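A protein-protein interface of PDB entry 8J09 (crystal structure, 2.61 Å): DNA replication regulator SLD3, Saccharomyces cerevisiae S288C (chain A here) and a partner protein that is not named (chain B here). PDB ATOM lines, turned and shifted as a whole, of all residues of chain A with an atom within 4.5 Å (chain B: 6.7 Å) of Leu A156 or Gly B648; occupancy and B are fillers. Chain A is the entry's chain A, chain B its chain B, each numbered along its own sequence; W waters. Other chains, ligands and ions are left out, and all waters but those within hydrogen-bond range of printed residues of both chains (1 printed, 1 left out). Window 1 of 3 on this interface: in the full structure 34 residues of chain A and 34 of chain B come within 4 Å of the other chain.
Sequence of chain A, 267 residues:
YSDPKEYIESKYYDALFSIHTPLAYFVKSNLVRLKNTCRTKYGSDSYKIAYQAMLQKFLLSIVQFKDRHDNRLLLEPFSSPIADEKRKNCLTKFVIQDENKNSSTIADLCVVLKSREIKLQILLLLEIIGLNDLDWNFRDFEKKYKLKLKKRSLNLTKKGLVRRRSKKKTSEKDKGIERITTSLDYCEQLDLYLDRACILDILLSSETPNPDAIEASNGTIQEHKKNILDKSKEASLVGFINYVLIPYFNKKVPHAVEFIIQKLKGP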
ATOM      1  N   LYS A 151       3.051   9.181 -23.153  1.00  0.00           N
ATOM      2  CA  LYS A 151       3.911   8.672 -24.218  1.00  0.00           C
ATOM      3  C   LYS A 151       4.950   7.705 -23.666  1.00  0.00           C
ATOM      4  O   LYS A 151       5.211   6.656 -24.264  1.00  0.00           O
ATOM      5  CB  LYS A 151       4.599   9.831 -24.942  1.00  0.00           C
ATOM      6  CG  LYS A 151       3.654  10.827 -25.588  1.00  0.00           C
ATOM      7  CD  LYS A 151       4.403  11.733 -26.555  1.00  0.00           C
ATOM      8  CE  LYS A 151       3.550  12.915 -26.989  1.00  0.00           C
ATOM      9  NZ  LYS A 151       3.422  13.935 -25.909  1.00  0.00           N
ATOM     10  N   ARG A 152       5.548   8.041 -22.520  1.00  0.00           N
ATOM     11  CA  ARG A 152       6.569   7.179 -21.935  1.00  0.00           C
ATOM     12  C   ARG A 152       5.979   5.845 -21.492  1.00  0.00           C
ATOM     13  O   ARG A 152       6.596   4.792 -21.692  1.00  0.00           O
ATOM     14  CB  ARG A 152       7.240   7.889 -20.760  1.00  0.00           C
ATOM     15  CG  ARG A 152       8.007   9.143 -21.154  1.00  0.00           C
ATOM     16  CD  ARG A 152       8.586   9.852 -19.940  1.00  0.00           C
ATOM     17  NE  ARG A 152       9.479   8.989 -19.170  1.00  0.00           N
ATOM     18  CZ  ARG A 152      10.288   9.421 -18.209  1.00  0.00           C
ATOM     19  NH1 ARG A 152      10.321  10.711 -17.897  1.00  0.00           N
ATOM     20  NH2 ARG A 152      11.066   8.566 -17.558  1.00  0.00           N
ATOM     21  N   SER A 153       4.784   5.872 -20.895  1.00  0.00           N
ATOM     22  CA  SER A 153       4.146   4.635 -20.456  1.00  0.00           C
ATOM     23  C   SER A 153       3.810   3.741 -21.641  1.00  0.00           C
ATOM     24  O   SER A 153       3.953   2.515 -21.565  1.00  0.00           O
ATOM     25  CB  SER A 153       2.886   4.951 -19.648  1.00  0.00           C
ATOM     26  OG  SER A 153       2.028   3.824 -19.575  1.00  0.00           O
ATOM     27  N   LEU A 154       3.358   4.338 -22.746  1.00  0.00           N
ATOM     28  CA  LEU A 154       3.105   3.559 -23.951  1.00  0.00           C
ATOM     29  C   LEU A 154       4.395   2.997 -24.534  1.00  0.00           C
ATOM     30  O   LEU A 154       4.393   1.890 -25.085  1.00  0.00           O
ATOM     31  CB  LEU A 154       2.385   4.417 -24.992  1.00  0.00           C
ATOM     32  CG  LEU A 154       0.951   4.843 -24.663  1.00  0.00           C
ATOM     33  CD1 LEU A 154       0.429   5.833 -25.697  1.00  0.00           C
ATOM     34  CD2 LEU A 154       0.036   3.632 -24.564  1.00  0.00           C
ATOM     35  N   ASN A 155       5.501   3.737 -24.415  1.00  0.00           N
ATOM     36  CA  ASN A 155       6.767   3.273 -24.973  1.00  0.00           C
ATOM     37  C   ASN A 155       7.319   2.076 -24.211  1.00  0.00           C
ATOM     38  O   ASN A 155       7.978   1.218 -24.808  1.00  0.00           O
ATOM     39  CB  ASN A 155       7.789   4.411 -24.982  1.00  0.00           C
ATOM     40  CG  ASN A 155       7.444   5.494 -25.982  1.00  0.00           C
ATOM     41  OD1 ASN A 155       6.664   5.273 -26.910  1.00  0.00           O
ATOM     42  ND2 ASN A 155       8.021   6.676 -25.799  1.00  0.00           N
ATOM     43  N   LEU A 156       7.074   2.004 -22.899  1.00  0.00           N
ATOM     44  CA  LEU A 156       7.476   0.826 -22.137  1.00  0.00           C
ATOM     45  C   LEU A 156       6.821  -0.434 -22.681  1.00  0.00           C
ATOM     46  O   LEU A 156       7.427  -1.512 -22.666  1.00  0.00           O
ATOM     47  CB  LEU A 156       7.121   1.005 -20.661  1.00  0.00           C
ATOM     48  CG  LEU A 156       7.901   2.070 -19.892  1.00  0.00           C
ATOM     49  CD1 LEU A 156       7.219   2.372 -18.566  1.00  0.00           C
ATOM     50  CD2 LEU A 156       9.338   1.621 -19.676  1.00  0.00           C
ATOM     51  N   THR A 157       5.587  -0.313 -23.173  1.00  0.00           N
ATOM     52  CA  THR A 157       4.871  -1.460 -23.714  1.00  0.00           C
ATOM     53  C   THR A 157       5.411  -1.875 -25.077  1.00  0.00           C
ATOM     54  O   THR A 157       5.390  -3.064 -25.414  1.00  0.00           O
ATOM     55  CB  THR A 157       3.382  -1.127 -23.813  1.00  0.00           C
ATOM     56  OG1 THR A 157       2.904  -0.681 -22.537  1.00  0.00           O
ATOM     57  CG2 THR A 157       2.588  -2.339 -24.247  1.00  0.00           C
ATOM     58  N   LYS A 158       5.916  -0.919 -25.860  1.00  0.00           N
ATOM     59  CA  LYS A 158       6.252  -1.177 -27.256  1.00  0.00           C
ATOM     60  C   LYS A 158       7.364  -2.207 -27.425  1.00  0.00           C
ATOM     61  O   LYS A 158       7.477  -2.805 -28.501  1.00  0.00           O
ATOM     62  CB  LYS A 158       6.648   0.131 -27.943  1.00  0.00           C
ATOM     63  CG  LYS A 158       5.708   0.553 -29.061  1.00  0.00           C
ATOM     64  CD  LYS A 158       5.899   2.017 -29.430  1.00  0.00           C
ATOM     65  CE  LYS A 158       4.956   2.914 -28.644  1.00  0.00           C
ATOM     66  NZ  LYS A 158       4.749   4.228 -29.314  1.00  0.00           N
ATOM     67  N   LYS A 159       8.182  -2.434 -26.396  1.00  0.00           N
ATOM     68  CA  LYS A 159       9.287  -3.379 -26.537  1.00  0.00           C
ATOM     69  C   LYS A 159       8.815  -4.824 -26.438  1.00  0.00           C
ATOM     70  O   LYS A 159       9.279  -5.683 -27.197  1.00  0.00           O
ATOM     71  CB  LYS A 159      10.357  -3.094 -25.484  1.00  0.00           C
ATOM     72  CG  LYS A 159      10.814  -1.647 -25.449  1.00  0.00           C
ATOM     73  CD  LYS A 159      10.733  -1.080 -24.046  1.00  0.00           C
ATOM     74  CE  LYS A 159      11.120   0.388 -24.025  1.00  0.00           C
ATOM     75  NZ  LYS A 159      11.145   0.930 -22.640  1.00  0.00           N
ATOM     76  N   SER B 242      -0.549  -1.132 -21.622  1.00  0.00           N
ATOM     77  CA  SER B 242       0.070  -0.094 -20.810  1.00  0.00           C
ATOM     78  C   SER B 242      -0.693   0.180 -19.525  1.00  0.00           C
ATOM     79  O   SER B 242      -0.199   0.931 -18.677  1.00  0.00           O
ATOM     80  CB  SER B 242       0.200   1.213 -21.609  1.00  0.00           C
ATOM     81  OG  SER B 242       1.009   1.025 -22.756  1.00  0.00           O
ATOM     82  N   LEU B 602       1.300   7.017 -15.694  1.00  0.00           N
ATOM     83  CA  LEU B 602       2.250   5.933 -15.921  1.00  0.00           C
ATOM     84  C   LEU B 602       1.969   4.845 -14.888  1.00  0.00           C
ATOM     85  O   LEU B 602       2.634   4.732 -13.858  1.00  0.00           O
ATOM     86  CB  LEU B 602       3.684   6.446 -15.841  1.00  0.00           C
ATOM     87  CG  LEU B 602       4.781   5.486 -16.303  1.00  0.00           C
ATOM     88  CD1 LEU B 602       5.646   6.142 -17.367  1.00  0.00           C
ATOM     89  CD2 LEU B 602       5.628   5.032 -15.126  1.00  0.00           C
ATOM     90  N   ASN B 604       2.140   1.581 -15.490  1.00  0.00           N
ATOM     91  CA  ASN B 604       2.946   0.385 -15.740  1.00  0.00           C
ATOM     92  C   ASN B 604       4.390   0.593 -15.305  1.00  0.00           C
ATOM     93  O   ASN B 604       5.330   0.256 -16.024  1.00  0.00           O
ATOM     94  CB  ASN B 604       2.868  -0.001 -17.212  1.00  0.00           C
ATOM     95  CG  ASN B 604       3.257   1.138 -18.131  1.00  0.00           C
ATOM     96  OD1 ASN B 604       2.982   2.303 -17.844  1.00  0.00           O
ATOM     97  ND2 ASN B 604       3.898   0.808 -19.245  1.00  0.00           N
ATOM     98  N   PHE B 605       4.581   1.158 -14.110  1.00  0.00           N
ATOM     99  CA  PHE B 605       5.935   1.379 -13.612  1.00  0.00           C
ATOM    100  C   PHE B 605       6.637   0.069 -13.287  1.00  0.00           C
ATOM    101  O   PHE B 605       7.856  -0.034 -13.459  1.00  0.00           O
ATOM    102  CB  PHE B 605       5.908   2.277 -12.376  1.00  0.00           C
ATOM    103  CG  PHE B 605       7.254   2.450 -11.727  1.00  0.00           C
ATOM    104  CD1 PHE B 605       8.153   3.389 -12.206  1.00  0.00           C
ATOM    105  CD2 PHE B 605       7.621   1.671 -10.639  1.00  0.00           C
ATOM    106  CE1 PHE B 605       9.392   3.550 -11.612  1.00  0.00           C
ATOM    107  CE2 PHE B 605       8.859   1.826 -10.042  1.00  0.00           C
ATOM    108  CZ  PHE B 605       9.746   2.767 -10.529  1.00  0.00           C
ATOM    109  N   MET B 607       6.525  -2.503 -14.961  1.00  0.00           N
ATOM    110  CA  MET B 607       7.115  -2.917 -16.229  1.00  0.00           C
ATOM    111  C   MET B 607       8.464  -2.245 -16.451  1.00  0.00           C
ATOM    112  O   MET B 607       9.420  -2.891 -16.895  1.00  0.00           O
ATOM    113  CB  MET B 607       6.154  -2.595 -17.374  1.00  0.00           C
ATOM    114  CG  MET B 607       6.428  -3.335 -18.668  1.00  0.00           C
ATOM    115  SD  MET B 607       5.221  -2.903 -19.939  1.00  0.00           S
ATOM    116  CE  MET B 607       3.687  -3.126 -19.040  1.00  0.00           C
ATOM    117  N   ALA B 608       8.559  -0.950 -16.145  1.00  0.00           N
ATOM    118  CA  ALA B 608       9.832  -0.247 -16.272  1.00  0.00           C
ATOM    119  C   ALA B 608      10.858  -0.771 -15.276  1.00  0.00           C
ATOM    120  O   ALA B 608      12.022  -0.987 -15.631  1.00  0.00           O
ATOM    121  CB  ALA B 608       9.623   1.254 -16.079  1.00  0.00           C
ATOM    122  N   PHE B 609      10.443  -0.976 -14.024  1.00  0.00           N
ATOM    123  CA  PHE B 609      11.361  -1.484 -13.011  1.00  0.00           C
ATOM    124  C   PHE B 609      11.887  -2.862 -13.391  1.00  0.00           C
ATOM    125  O   PHE B 609      13.059  -3.177 -13.151  1.00  0.00           O
ATOM    126  CB  PHE B 609      10.664  -1.531 -11.652  1.00  0.00           C
ATOM    127  CG  PHE B 609      11.605  -1.687 -10.497  1.00  0.00           C
ATOM    128  CD1 PHE B 609      12.116  -0.574  -9.846  1.00  0.00           C
ATOM    129  CD2 PHE B 609      11.987  -2.944 -10.066  1.00  0.00           C
ATOM    130  CE1 PHE B 609      12.987  -0.716  -8.781  1.00  0.00           C
ATOM    131  CE2 PHE B 609      12.860  -3.091  -9.008  1.00  0.00           C
ATOM    132  CZ  PHE B 609      13.358  -1.977  -8.361  1.00  0.00           C
ATOM    133  N   GLN B 611      12.293  -4.019 -16.470  1.00  0.00           N
ATOM    134  CA  GLN B 611      13.208  -3.903 -17.600  1.00  0.00           C
ATOM    135  C   GLN B 611      14.592  -3.438 -17.166  1.00  0.00           C
ATOM    136  O   GLN B 611      15.598  -3.869 -17.742  1.00  0.00           O
ATOM    137  CB  GLN B 611      12.626  -2.952 -18.647  1.00  0.00           C
ATOM    138  CG  GLN B 611      11.387  -3.495 -19.347  1.00  0.00           C
ATOM    139  CD  GLN B 611      10.723  -2.475 -20.256  1.00  0.00           C
ATOM    140  OE1 GLN B 611      11.072  -1.295 -20.245  1.00  0.00           O
ATOM    141  NE2 GLN B 611       9.758  -2.929 -21.048  1.00  0.00           N
ATOM    142  N   LYS B 643      19.108   5.101 -14.692  1.00  0.00           N
ATOM    143  CA  LYS B 643      18.379   4.505 -15.808  1.00  0.00           C
ATOM    144  C   LYS B 643      16.875   4.530 -15.572  1.00  0.00           C
ATOM    145  O   LYS B 643      16.100   4.663 -16.527  1.00  0.00           O
ATOM    146  CB  LYS B 643      18.840   3.065 -16.039  1.00  0.00           C
ATOM    147  CG  LYS B 643      20.286   2.911 -16.468  1.00  0.00           C
ATOM    148  CD  LYS B 643      20.594   1.455 -16.777  1.00  0.00           C
ATOM    149  CE  LYS B 643      22.074   1.145 -16.634  1.00  0.00           C
ATOM    150  NZ  LYS B 643      22.353  -0.296 -16.889  1.00  0.00           N
ATOM    151  N   LEU B 644      16.447   4.401 -14.314  1.00  0.00           N
ATOM    152  CA  LEU B 644      15.020   4.374 -14.007  1.00  0.00           C
ATOM    153  C   LEU B 644      14.347   5.688 -14.385  1.00  0.00           C
ATOM    154  O   LEU B 644      13.194   5.697 -14.833  1.00  0.00           O
ATOM    155  CB  LEU B 644      14.818   4.068 -12.523  1.00  0.00           C
ATOM    156  CG  LEU B 644      13.644   3.175 -12.117  1.00  0.00           C
ATOM    157  CD1 LEU B 644      13.406   2.083 -13.144  1.00  0.00           C
ATOM    158  CD2 LEU B 644      13.901   2.573 -10.744  1.00  0.00           C
ATOM    159  N   THR B 645      15.054   6.809 -14.221  1.00  0.00           N
ATOM    160  CA  THR B 645      14.487   8.109 -14.561  1.00  0.00           C
ATOM    161  C   THR B 645      14.288   8.286 -16.061  1.00  0.00           C
ATOM    162  O   THR B 645      13.567   9.202 -16.473  1.00  0.00           O
ATOM    163  CB  THR B 645      15.381   9.231 -14.034  1.00  0.00           C
ATOM    164  OG1 THR B 645      16.563   9.318 -14.840  1.00  0.00           O
ATOM    165  CG2 THR B 645      15.775   8.964 -12.594  1.00  0.00           C
ATOM    166  N   LEU B 646      14.908   7.443 -16.884  1.00  0.00           N
ATOM    167  CA  LEU B 646      14.791   7.534 -18.331  1.00  0.00           C
ATOM    168  C   LEU B 646      13.773   6.555 -18.900  1.00  0.00           C
ATOM    169  O   LEU B 646      13.732   6.362 -20.119  1.00  0.00           O
ATOM    170  CB  LEU B 646      16.155   7.304 -18.986  1.00  0.00           C
ATOM    171  CG  LEU B 646      17.338   8.111 -18.447  1.00  0.00           C
ATOM    172  CD1 LEU B 646      18.608   7.772 -19.211  1.00  0.00           C
ATOM    173  CD2 LEU B 646      17.054   9.604 -18.517  1.00  0.00           C
ATOM    174  N   SER B 647      12.952   5.941 -18.050  1.00  0.00           N
ATOM    175  CA  SER B 647      12.029   4.907 -18.500  1.00  0.00           C
ATOM    176  C   SER B 647      11.034   5.463 -19.511  1.00  0.00           C
ATOM    177  O   SER B 647      10.387   6.486 -19.268  1.00  0.00           O
ATOM    178  CB  SER B 647      11.286   4.315 -17.303  1.00  0.00           C
ATOM    179  OG  SER B 647      12.188   3.716 -16.389  1.00  0.00           O
ATOM    180  N   GLY B 648      10.919   4.783 -20.650  1.00  0.00           N
ATOM    181  CA  GLY B 648       9.973   5.167 -21.681  1.00  0.00           C
ATOM    182  C   GLY B 648      10.342   6.392 -22.485  1.00  0.00           C
ATOM    183  O   GLY B 648       9.495   6.909 -23.219  1.00  0.00           O
ATOM    184  N   LEU B 649      11.582   6.870 -22.385  1.00  0.00           N
ATOM    185  CA  LEU B 649      11.965   8.093 -23.086  1.00  0.00           C
ATOM    186  C   LEU B 649      12.275   7.823 -24.555  1.00  0.00           C
ATOM    187  O   LEU B 649      11.648   8.401 -25.449  1.00  0.00           O
ATOM    188  CB  LEU B 649      13.167   8.740 -22.395  1.00  0.00           C
ATOM    189  CG  LEU B 649      12.828   9.709 -21.263  1.00  0.00           C
ATOM    190  CD1 LEU B 649      14.098  10.284 -20.664  1.00  0.00           C
ATOM    191  CD2 LEU B 649      11.913  10.816 -21.764  1.00  0.00           C
ATOM    192  N   LEU B 650      13.244   6.953 -24.819  1.00  0.00           N
ATOM    193  CA  LEU B 650      13.695   6.706 -26.185  1.00  0.00           C
ATOM    194  C   LEU B 650      13.152   5.386 -26.721  1.00  0.00           C
ATOM    195  O   LEU B 650      12.991   5.217 -27.930  1.00  0.00           O
ATOM    196  CB  LEU B 650      15.225   6.712 -26.252  1.00  0.00           C
ATOM    197  CG  LEU B 650      15.923   8.056 -26.490  1.00  0.00           C
ATOM    198  CD1 LEU B 650      15.624   9.054 -25.376  1.00  0.00           C
ATOM    199  CD2 LEU B 650      17.424   7.857 -26.641  1.00  0.00           C
HETATM  200  O   HOH W   1      11.898  11.426 -15.711  1.00  0.00           O
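NH2 of Arg A152 lies within hydrogen-bond range of O of Thr B645, 2.8 Å away.
The guanidinium group (NE) of Arg A152 sits at hydrogen-bond distance from the backbone carbonyl oxygen (O) of Ser B647.
The side-chain hydroxyl of Ser A153 is in hydrogen-bond range of the side-chain amide oxygen of Asn B604, 2.5 Å away.
ND2 of Asn A155 sits at hydrogen-bond distance from O of Gly B648.
O of Leu A156 is in hydrogen-bond range of NE2 of Gln B611, at 3.2 Å.
The side-chain hydroxyl of Ser B242 sits at hydrogen-bond distance from the side-chain hydroxyl of Thr A157 (2.6 Å).
The side-chain amide oxygen (OE1) of Gln B611 is in hydrogen-bond range of the side-chain amino group (NZ) of Lys A159.
The backbone carbonyl oxygen of Leu A156 sits close to the side-chain sulfur of Met B607 (3.8 Å).
The backbone carbonyl oxygen (O) of Lys A151 sits close to the side-chain amide nitrogen (ND2) of Asn A155, 3.2 Å away.
OD1 of Asn A155 lies within hydrogen-bond range of NZ of Lys A158.
OG of Ser B647 is in hydrogen-bond range of O of Leu B644.
Among the printed residues, pairs that only touch across the chains: Arg A152 with Leu B646, Arg A152 with Gly B648, Arg A152 with Leu B649, Ser A153 with Ser B242, Ser A153 with Leu B602, Leu A154 with Ser B242, Leu A156 with Asn B604, Leu A156 with Ala B608, Leu A156 with Gly B648 and Thr A157 with Asn B604.
Leu A156 touches just these residues of chain B: Asn B604 (3.5 Å), Met B607 (3.8 Å), Ala B608 (3.6 Å), Gln B611 (3.2 Å) and Gly B648 (3.7 Å).
Printed residues of chain B within 4 Å of Thr A157: Ser B242 and Asn B604.
Of the printed residues of chain A, Gln B611 touches Leu A156 and Lys A159.
Of the printed residues of chain B, Leu A154 touches Ser B242 (3.3 Å).
Printed residues of chain B within 4 Å of Ser A153: Ser B242, Leu B602 and Asn B604.
Printed residues of chain A within 4 Å of Ser B242: Ser A153 (3.5 Å), Leu A154 (3.3 Å) and Thr A157 (2.6 Å).
Leu B650 touches none of the printed residues of chain A.
The nearest residue of chain B that does not touch Leu A156 is Ser B647 (4.1 Å).
The nearest printed residue of chain A that does not touch Ser B242 is Asn A155 (5.5 Å).
Printed residues of chain A that touch a printed residue of chain B: Arg A152, Ser A153, Leu A154, Asn A155, Leu A156, Thr A157 and Lys A159.
Hydrophobic or aromatic side chains of chain A within 4 Å of the printed part of chain B: Leu A154 and Leu A156.
Hydrophobic or aromatic side chains of chain B that line the printed part of chain A: Leu B602, Met B607, Ala B608 and Leu B649.
Among the printed residues, 18 pairs touch across the chains.
Among the printed residues, no Asp or Glu carboxylate lies within 4 Å of a Lys or Arg side-chain nitrogen of the other chain.
Water W1 bridges the guanidinium group (NH1) of Arg A152 and the backbone carbonyl oxygen (O) of Thr B645.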
